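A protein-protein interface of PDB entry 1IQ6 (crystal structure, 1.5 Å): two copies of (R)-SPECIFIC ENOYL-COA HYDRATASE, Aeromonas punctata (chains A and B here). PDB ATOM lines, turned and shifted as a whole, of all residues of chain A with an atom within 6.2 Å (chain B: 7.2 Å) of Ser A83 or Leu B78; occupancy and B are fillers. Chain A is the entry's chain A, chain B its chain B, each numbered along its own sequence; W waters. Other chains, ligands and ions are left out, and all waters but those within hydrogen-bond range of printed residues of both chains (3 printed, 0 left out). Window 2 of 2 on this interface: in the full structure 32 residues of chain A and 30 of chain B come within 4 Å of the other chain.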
ATOM      1  N   SER A  81      10.593   2.840   9.045  1.00  0.00           N
ATOM      2  CA  SER A  81      11.462   2.225  10.046  1.00  0.00           C
ATOM      3  C   SER A  81      12.275   3.355  10.667  1.00  0.00           C
ATOM      4  O   SER A  81      12.650   4.311   9.980  1.00  0.00           O
ATOM      5  CB  SER A  81      12.388   1.175   9.416  1.00  0.00           C
ATOM      6  OG  SER A  81      13.223   1.738   8.421  1.00  0.00           O
ATOM      7  N   LEU A  82      12.546   3.247  11.961  1.00  0.00           N
ATOM      8  CA  LEU A  82      13.277   4.293  12.654  1.00  0.00           C
ATOM      9  C   LEU A  82      14.316   3.783  13.641  1.00  0.00           C
ATOM     10  O   LEU A  82      14.030   2.937  14.485  1.00  0.00           O
ATOM     11  CB  LEU A  82      12.295   5.192  13.409  1.00  0.00           C
ATOM     12  CG  LEU A  82      11.227   5.910  12.589  1.00  0.00           C
ATOM     13  CD1 LEU A  82      10.151   6.440  13.525  1.00  0.00           C
ATOM     14  CD2 LEU A  82      11.862   7.028  11.778  1.00  0.00           C
ATOM     15  N   SER A  83      15.527   4.312  13.517  1.00  0.00           N
ATOM     16  CA  SER A  83      16.616   3.973  14.421  1.00  0.00           C
ATOM     17  C   SER A  83      17.079   5.297  15.009  1.00  0.00           C
ATOM     18  O   SER A  83      17.493   6.200  14.277  1.00  0.00           O
ATOM     19  CB  SER A  83      17.768   3.302  13.675  1.00  0.00           C
ATOM     20  OG  SER A  83      17.422   1.983  13.287  1.00  0.00           O
ATOM     21  N   PHE A  84      16.978   5.422  16.327  1.00  0.00           N
ATOM     22  CA  PHE A  84      17.384   6.642  17.004  1.00  0.00           C
ATOM     23  C   PHE A  84      18.820   6.450  17.487  1.00  0.00           C
ATOM     24  O   PHE A  84      19.089   5.641  18.375  1.00  0.00           O
ATOM     25  CB  PHE A  84      16.417   6.933  18.154  1.00  0.00           C
ATOM     26  CG  PHE A  84      14.972   7.024  17.713  1.00  0.00           C
ATOM     27  CD1 PHE A  84      14.100   5.955  17.902  1.00  0.00           C
ATOM     28  CD2 PHE A  84      14.500   8.165  17.072  1.00  0.00           C
ATOM     29  CE1 PHE A  84      12.775   6.022  17.459  1.00  0.00           C
ATOM     30  CE2 PHE A  84      13.176   8.244  16.624  1.00  0.00           C
ATOM     31  CZ  PHE A  84      12.312   7.169  16.819  1.00  0.00           C
ATOM     32  N   LYS A  85      19.736   7.204  16.890  1.00  0.00           N
ATOM     33  CA  LYS A  85      21.161   7.077  17.188  1.00  0.00           C
ATOM     34  C   LYS A  85      21.763   8.109  18.130  1.00  0.00           C
ATOM     35  O   LYS A  85      22.532   7.763  19.029  1.00  0.00           O
ATOM     36  CB  LYS A  85      21.955   7.116  15.878  1.00  0.00           C
ATOM     37  CG  LYS A  85      21.415   6.238  14.756  1.00  0.00           C
ATOM     38  CD  LYS A  85      21.607   4.758  15.037  1.00  0.00           C
ATOM     39  CE  LYS A  85      21.238   3.926  13.817  1.00  0.00           C
ATOM     40  NZ  LYS A  85      21.490   2.470  14.023  1.00  0.00           N
ATOM     41  N   ALA A 124      21.515  11.390  13.411  1.00  0.00           N
ATOM     42  CA  ALA A 124      20.703  11.255  14.617  1.00  0.00           C
ATOM     43  C   ALA A 124      19.572  10.234  14.489  1.00  0.00           C
ATOM     44  O   ALA A 124      19.254   9.528  15.443  1.00  0.00           O
ATOM     45  CB  ALA A 124      20.128  12.611  15.009  1.00  0.00           C
ATOM     46  N   VAL A 125      18.958  10.169  13.313  1.00  0.00           N
ATOM     47  CA  VAL A 125      17.864   9.234  13.070  1.00  0.00           C
ATOM     48  C   VAL A 125      18.000   8.690  11.659  1.00  0.00           C
ATOM     49  O   VAL A 125      18.292   9.436  10.730  1.00  0.00           O
ATOM     50  CB  VAL A 125      16.478   9.929  13.182  1.00  0.00           C
ATOM     51  CG1 VAL A 125      15.358   8.904  12.991  1.00  0.00           C
ATOM     52  CG2 VAL A 125      16.343  10.614  14.529  1.00  0.00           C
ATOM     53  N   THR A 126      17.795   7.390  11.489  1.00  0.00           N
ATOM     54  CA  THR A 126      17.891   6.815  10.161  1.00  0.00           C
ATOM     55  C   THR A 126      16.848   5.725   9.988  1.00  0.00           C
ATOM     56  O   THR A 126      16.359   5.160  10.964  1.00  0.00           O
ATOM     57  CB  THR A 126      19.308   6.239   9.897  1.00  0.00           C
ATOM     58  OG1 THR A 126      19.436   5.904   8.508  1.00  0.00           O
ATOM     59  CG2 THR A 126      19.554   4.999  10.744  1.00  0.00           C
ATOM     60  N   GLY A 127      16.497   5.454   8.741  1.00  0.00           N
ATOM     61  CA  GLY A 127      15.511   4.433   8.458  1.00  0.00           C
ATOM     62  C   GLY A 127      15.057   4.517   7.019  1.00  0.00           C
ATOM     63  O   GLY A 127      15.696   5.173   6.194  1.00  0.00           O
ATOM     64  N   ILE B  76      14.354   5.172  27.098  1.00  0.00           N
ATOM     65  CA  ILE B  76      14.960   5.846  25.961  1.00  0.00           C
ATOM     66  C   ILE B  76      14.668   5.066  24.678  1.00  0.00           C
ATOM     67  O   ILE B  76      14.918   3.867  24.597  1.00  0.00           O
ATOM     68  CB  ILE B  76      16.488   5.986  26.145  1.00  0.00           C
ATOM     69  CG1 ILE B  76      16.783   6.882  27.353  1.00  0.00           C
ATOM     70  CG2 ILE B  76      17.114   6.561  24.884  1.00  0.00           C
ATOM     71  CD1 ILE B  76      18.258   7.032  27.666  1.00  0.00           C
ATOM     72  N   TYR B  77      14.122   5.762  23.687  1.00  0.00           N
ATOM     73  CA  TYR B  77      13.779   5.175  22.394  1.00  0.00           C
ATOM     74  C   TYR B  77      15.028   4.785  21.607  1.00  0.00           C
ATOM     75  O   TYR B  77      15.909   5.614  21.384  1.00  0.00           O
ATOM     76  CB  TYR B  77      12.988   6.200  21.577  1.00  0.00           C
ATOM     77  CG  TYR B  77      11.617   5.772  21.090  1.00  0.00           C
ATOM     78  CD1 TYR B  77      10.600   6.716  20.965  1.00  0.00           C
ATOM     79  CD2 TYR B  77      11.353   4.460  20.689  1.00  0.00           C
ATOM     80  CE1 TYR B  77       9.358   6.378  20.454  1.00  0.00           C
ATOM     81  CE2 TYR B  77      10.097   4.107  20.169  1.00  0.00           C
ATOM     82  CZ  TYR B  77       9.108   5.081  20.056  1.00  0.00           C
ATOM     83  OH  TYR B  77       7.867   4.781  19.544  1.00  0.00           O
ATOM     84  N   LEU B  78      15.108   3.527  21.186  1.00  0.00           N
ATOM     85  CA  LEU B  78      16.240   3.071  20.387  1.00  0.00           C
ATOM     86  C   LEU B  78      15.776   2.803  18.953  1.00  0.00           C
ATOM     87  O   LEU B  78      16.519   3.015  17.997  1.00  0.00           O
ATOM     88  CB  LEU B  78      16.857   1.799  20.982  1.00  0.00           C
ATOM     89  CG  LEU B  78      17.493   1.916  22.371  1.00  0.00           C
ATOM     90  CD1 LEU B  78      18.117   0.580  22.746  1.00  0.00           C
ATOM     91  CD2 LEU B  78      18.553   3.009  22.383  1.00  0.00           C
ATOM     92  N   GLY B  79      14.537   2.339  18.802  1.00  0.00           N
ATOM     93  CA  GLY B  79      14.023   2.066  17.474  1.00  0.00           C
ATOM     94  C   GLY B  79      12.522   1.865  17.449  1.00  0.00           C
ATOM     95  O   GLY B  79      11.916   1.526  18.464  1.00  0.00           O
ATOM     96  N   GLN B  80      11.921   2.089  16.286  1.00  0.00           N
ATOM     97  CA  GLN B  80      10.484   1.910  16.116  1.00  0.00           C
ATOM     98  C   GLN B  80      10.180   1.558  14.672  1.00  0.00           C
ATOM     99  O   GLN B  80      10.592   2.272  13.758  1.00  0.00           O
ATOM    100  CB  GLN B  80       9.725   3.190  16.490  1.00  0.00           C
ATOM    101  CG  GLN B  80       8.213   3.122  16.243  1.00  0.00           C
ATOM    102  CD  GLN B  80       7.477   2.230  17.237  1.00  0.00           C
ATOM    103  OE1 GLN B  80       7.484   2.488  18.443  1.00  0.00           O
ATOM    104  NE2 GLN B  80       6.832   1.183  16.730  1.00  0.00           N
ATOM    105  N   ARG B 104      16.164  -8.255  26.866  1.00  0.00           N
ATOM    106  CA  ARG B 104      17.537  -8.724  26.703  1.00  0.00           C
ATOM    107  C   ARG B 104      18.275  -8.799  28.030  1.00  0.00           C
ATOM    108  O   ARG B 104      17.987  -8.047  28.960  1.00  0.00           O
ATOM    109  CB  ARG B 104      18.284  -7.817  25.726  1.00  0.00           C
ATOM    110  CG  ARG B 104      17.864  -8.046  24.286  1.00  0.00           C
ATOM    111  CD  ARG B 104      18.439  -7.012  23.341  1.00  0.00           C
ATOM    112  NE  ARG B 104      19.895  -6.953  23.381  1.00  0.00           N
ATOM    113  CZ  ARG B 104      20.626  -6.222  22.545  1.00  0.00           C
ATOM    114  NH1 ARG B 104      21.948  -6.216  22.646  1.00  0.00           N
ATOM    115  NH2 ARG B 104      20.034  -5.503  21.601  1.00  0.00           N
ATOM    116  N   LYS B 107      22.064  -6.470  27.831  1.00  0.00           N
ATOM    117  CA  LYS B 107      21.884  -5.032  28.019  1.00  0.00           C
ATOM    118  C   LYS B 107      20.441  -4.780  28.451  1.00  0.00           C
ATOM    119  O   LYS B 107      19.544  -5.546  28.101  1.00  0.00           O
ATOM    120  CB  LYS B 107      22.158  -4.272  26.716  1.00  0.00           C
ATOM    121  CG  LYS B 107      23.570  -4.429  26.171  1.00  0.00           C
ATOM    122  CD  LYS B 107      23.851  -3.427  25.057  1.00  0.00           C
ATOM    123  CE  LYS B 107      22.928  -3.626  23.869  1.00  0.00           C
ATOM    124  NZ  LYS B 107      23.136  -2.586  22.822  1.00  0.00           N
ATOM    125  N   PRO B 108      20.200  -3.705  29.221  1.00  0.00           N
ATOM    126  CA  PRO B 108      18.852  -3.369  29.691  1.00  0.00           C
ATOM    127  C   PRO B 108      17.997  -2.790  28.566  1.00  0.00           C
ATOM    128  O   PRO B 108      17.711  -1.591  28.534  1.00  0.00           O
ATOM    129  CB  PRO B 108      19.123  -2.357  30.798  1.00  0.00           C
ATOM    130  CG  PRO B 108      20.310  -1.629  30.271  1.00  0.00           C
ATOM    131  CD  PRO B 108      21.190  -2.758  29.765  1.00  0.00           C
ATOM    132  N   ILE B 109      17.595  -3.659  27.648  1.00  0.00           N
ATOM    133  CA  ILE B 109      16.789  -3.266  26.501  1.00  0.00           C
ATOM    134  C   ILE B 109      15.533  -4.125  26.416  1.00  0.00           C
ATOM    135  O   ILE B 109      15.565  -5.318  26.714  1.00  0.00           O
ATOM    136  CB  ILE B 109      17.604  -3.414  25.199  1.00  0.00           C
ATOM    137  CG1 ILE B 109      18.779  -2.431  25.220  1.00  0.00           C
ATOM    138  CG2 ILE B 109      16.710  -3.188  23.979  1.00  0.00           C
ATOM    139  CD1 ILE B 109      19.689  -2.519  24.013  1.00  0.00           C
ATOM    140  N   ALA B 110      14.425  -3.512  26.013  1.00  0.00           N
ATOM    141  CA  ALA B 110      13.169  -4.229  25.887  1.00  0.00           C
ATOM    142  C   ALA B 110      12.584  -4.029  24.502  1.00  0.00           C
ATOM    143  O   ALA B 110      12.791  -2.991  23.872  1.00  0.00           O
ATOM    144  CB  ALA B 110      12.169  -3.735  26.933  1.00  0.00           C
ATOM    145  N   ALA B 129       8.690  -1.547  19.027  1.00  0.00           N
ATOM    146  CA  ALA B 129       9.562  -0.535  19.592  1.00  0.00           C
ATOM    147  C   ALA B 129      10.683  -1.246  20.339  1.00  0.00           C
ATOM    148  O   ALA B 129      10.492  -2.332  20.892  1.00  0.00           O
ATOM    149  CB  ALA B 129       8.789   0.357  20.558  1.00  0.00           C
ATOM    150  N   VAL B 130      11.860  -0.639  20.320  1.00  0.00           N
ATOM    151  CA  VAL B 130      13.013  -1.158  21.042  1.00  0.00           C
ATOM    152  C   VAL B 130      13.403   0.011  21.937  1.00  0.00           C
ATOM    153  O   VAL B 130      13.647   1.115  21.448  1.00  0.00           O
ATOM    154  CB  VAL B 130      14.182  -1.499  20.098  1.00  0.00           C
ATOM    155  CG1 VAL B 130      15.375  -1.982  20.917  1.00  0.00           C
ATOM    156  CG2 VAL B 130      13.758  -2.582  19.111  1.00  0.00           C
ATOM    157  N   VAL B 131      13.450  -0.225  23.245  1.00  0.00           N
ATOM    158  CA  VAL B 131      13.767   0.846  24.180  1.00  0.00           C
ATOM    159  C   VAL B 131      14.757   0.467  25.270  1.00  0.00           C
ATOM    160  O   VAL B 131      14.786  -0.674  25.737  1.00  0.00           O
ATOM    161  CB  VAL B 131      12.486   1.362  24.879  1.00  0.00           C
ATOM    162  CG1 VAL B 131      11.471   1.816  23.846  1.00  0.00           C
ATOM    163  CG2 VAL B 131      11.894   0.270  25.746  1.00  0.00           C
ATOM    164  N   LYS B 132      15.565   1.445  25.666  1.00  0.00           N
ATOM    165  CA  LYS B 132      16.544   1.264  26.732  1.00  0.00           C
ATOM    166  C   LYS B 132      15.775   1.475  28.035  1.00  0.00           C
ATOM    167  O   LYS B 132      15.046   2.458  28.180  1.00  0.00           O
ATOM    168  CB  LYS B 132      17.661   2.300  26.602  1.00  0.00           C
ATOM    169  CG  LYS B 132      18.770   2.161  27.636  1.00  0.00           C
ATOM    170  CD  LYS B 132      19.834   3.235  27.456  1.00  0.00           C
ATOM    171  CE  LYS B 132      20.504   3.131  26.095  1.00  0.00           C
ATOM    172  NZ  LYS B 132      21.545   4.180  25.908  1.00  0.00           N
ATOM    173  N   LEU B 133      15.934   0.551  28.974  1.00  0.00           N
ATOM    174  CA  LEU B 133      15.222   0.619  30.247  1.00  0.00           C
ATOM    175  C   LEU B 133      15.620   1.793  31.135  1.00  0.00           C
ATOM    176  O   LEU B 133      16.755   2.264  31.087  1.00  0.00           O
ATOM    177  CB  LEU B 133      15.411  -0.694  31.012  1.00  0.00           C
ATOM    178  CG  LEU B 133      14.959  -1.954  30.269  1.00  0.00           C
ATOM    179  CD1 LEU B 133      15.147  -3.171  31.163  1.00  0.00           C
ATOM    180  CD2 LEU B 133      13.502  -1.814  29.857  1.00  0.00           C
HETATM  181  O   HOH W   1      18.557   6.297  21.375  1.00  0.00           O
HETATM  182  O   HOH W   2      12.827   0.174  13.426  1.00  0.00           O
HETATM  183  O   HOH W   3      19.282   2.891  18.007  1.00  0.00           O
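N of Leu A82 is in hydrogen-bond range of O of Gln B80 (2.8 Å).
O of Leu B78 lies within hydrogen-bond range of N of Phe A84, at 3.0 Å.
The backbone carbonyl oxygen of Thr A126 is in hydrogen-bond range of the backbone NH of Ser A83 (2.8 Å).
The side-chain amide oxygen (OE1) of Gln B80 lies within hydrogen-bond range of the side-chain hydroxyl (OH) of Tyr B77 (2.6 Å).
The backbone NH of Leu B78 sits at hydrogen-bond distance from the backbone carbonyl oxygen of Val B130.
The backbone carbonyl oxygen (O) of Gly B79 sits at hydrogen-bond distance from the backbone NH (N) of Val B130, 2.9 Å away.
Among the printed residues, merely in contact across the chains: Ser A81 with Gln B80 (3.7 Å), Leu A82 with Gly B79 (3.1 Å), Ser A83 with Leu B78 (3.7 Å), Phe A84 with Tyr B77 (3.5 Å) and Phe A84 with Gly B79 (3.8 Å).
Of the printed residues of chain B, Ser A81 touches Gln B80 (3.7 Å).
Ser A83 touches one residue of chain B.
Thr A126 touches none of the printed residues of chain B.
Of chain A, only Ser A83 (3.7 Å) and Phe A84 (3.0 Å) come within 4 Å of Leu B78.
Printed residues of chain A within 4 Å of Gly B79: Leu A82 (3.1 Å) and Phe A84 (3.8 Å).
The nearest residue of chain A that does not touch Leu B78 is Leu A82 (4.3 Å).
Of the 9 printed residues of chain A, 4 touch a printed residue of chain B.
Printed residues of chain A that touch a printed residue of chain B: Ser A81, Leu A82, Ser A83 and Phe A84.
Hydrophobic or aromatic side chains of chain A that line the printed part of chain B: Leu A82 and Phe A84.
Printed residues of chain B that touch a printed residue of chain A: Tyr B77, Leu B78, Gly B79 and Gln B80.
Hydrophobic or aromatic side chains of chain B within 4 Å of the printed part of chain A: Tyr B77.
Among the printed residues, no Asp or Glu carboxylate lies within 4 Å of a Lys or Arg side-chain nitrogen of the other chain.
No position is printed for both chains.
Water W1 bridges the backbone carbonyl oxygen (O) of Tyr B77 (2.7 Å) and the backbone carbonyl oxygen (O) of Phe A84 (3.1 Å).
Water W3 bridges the backbone carbonyl oxygen of Leu B78 and the backbone carbonyl oxygen of Phe A84.
Water W2 lies within hydrogen-bond range of the backbone carbonyl oxygen of Gln B80 and the backbone carbonyl oxygen of Leu A82.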
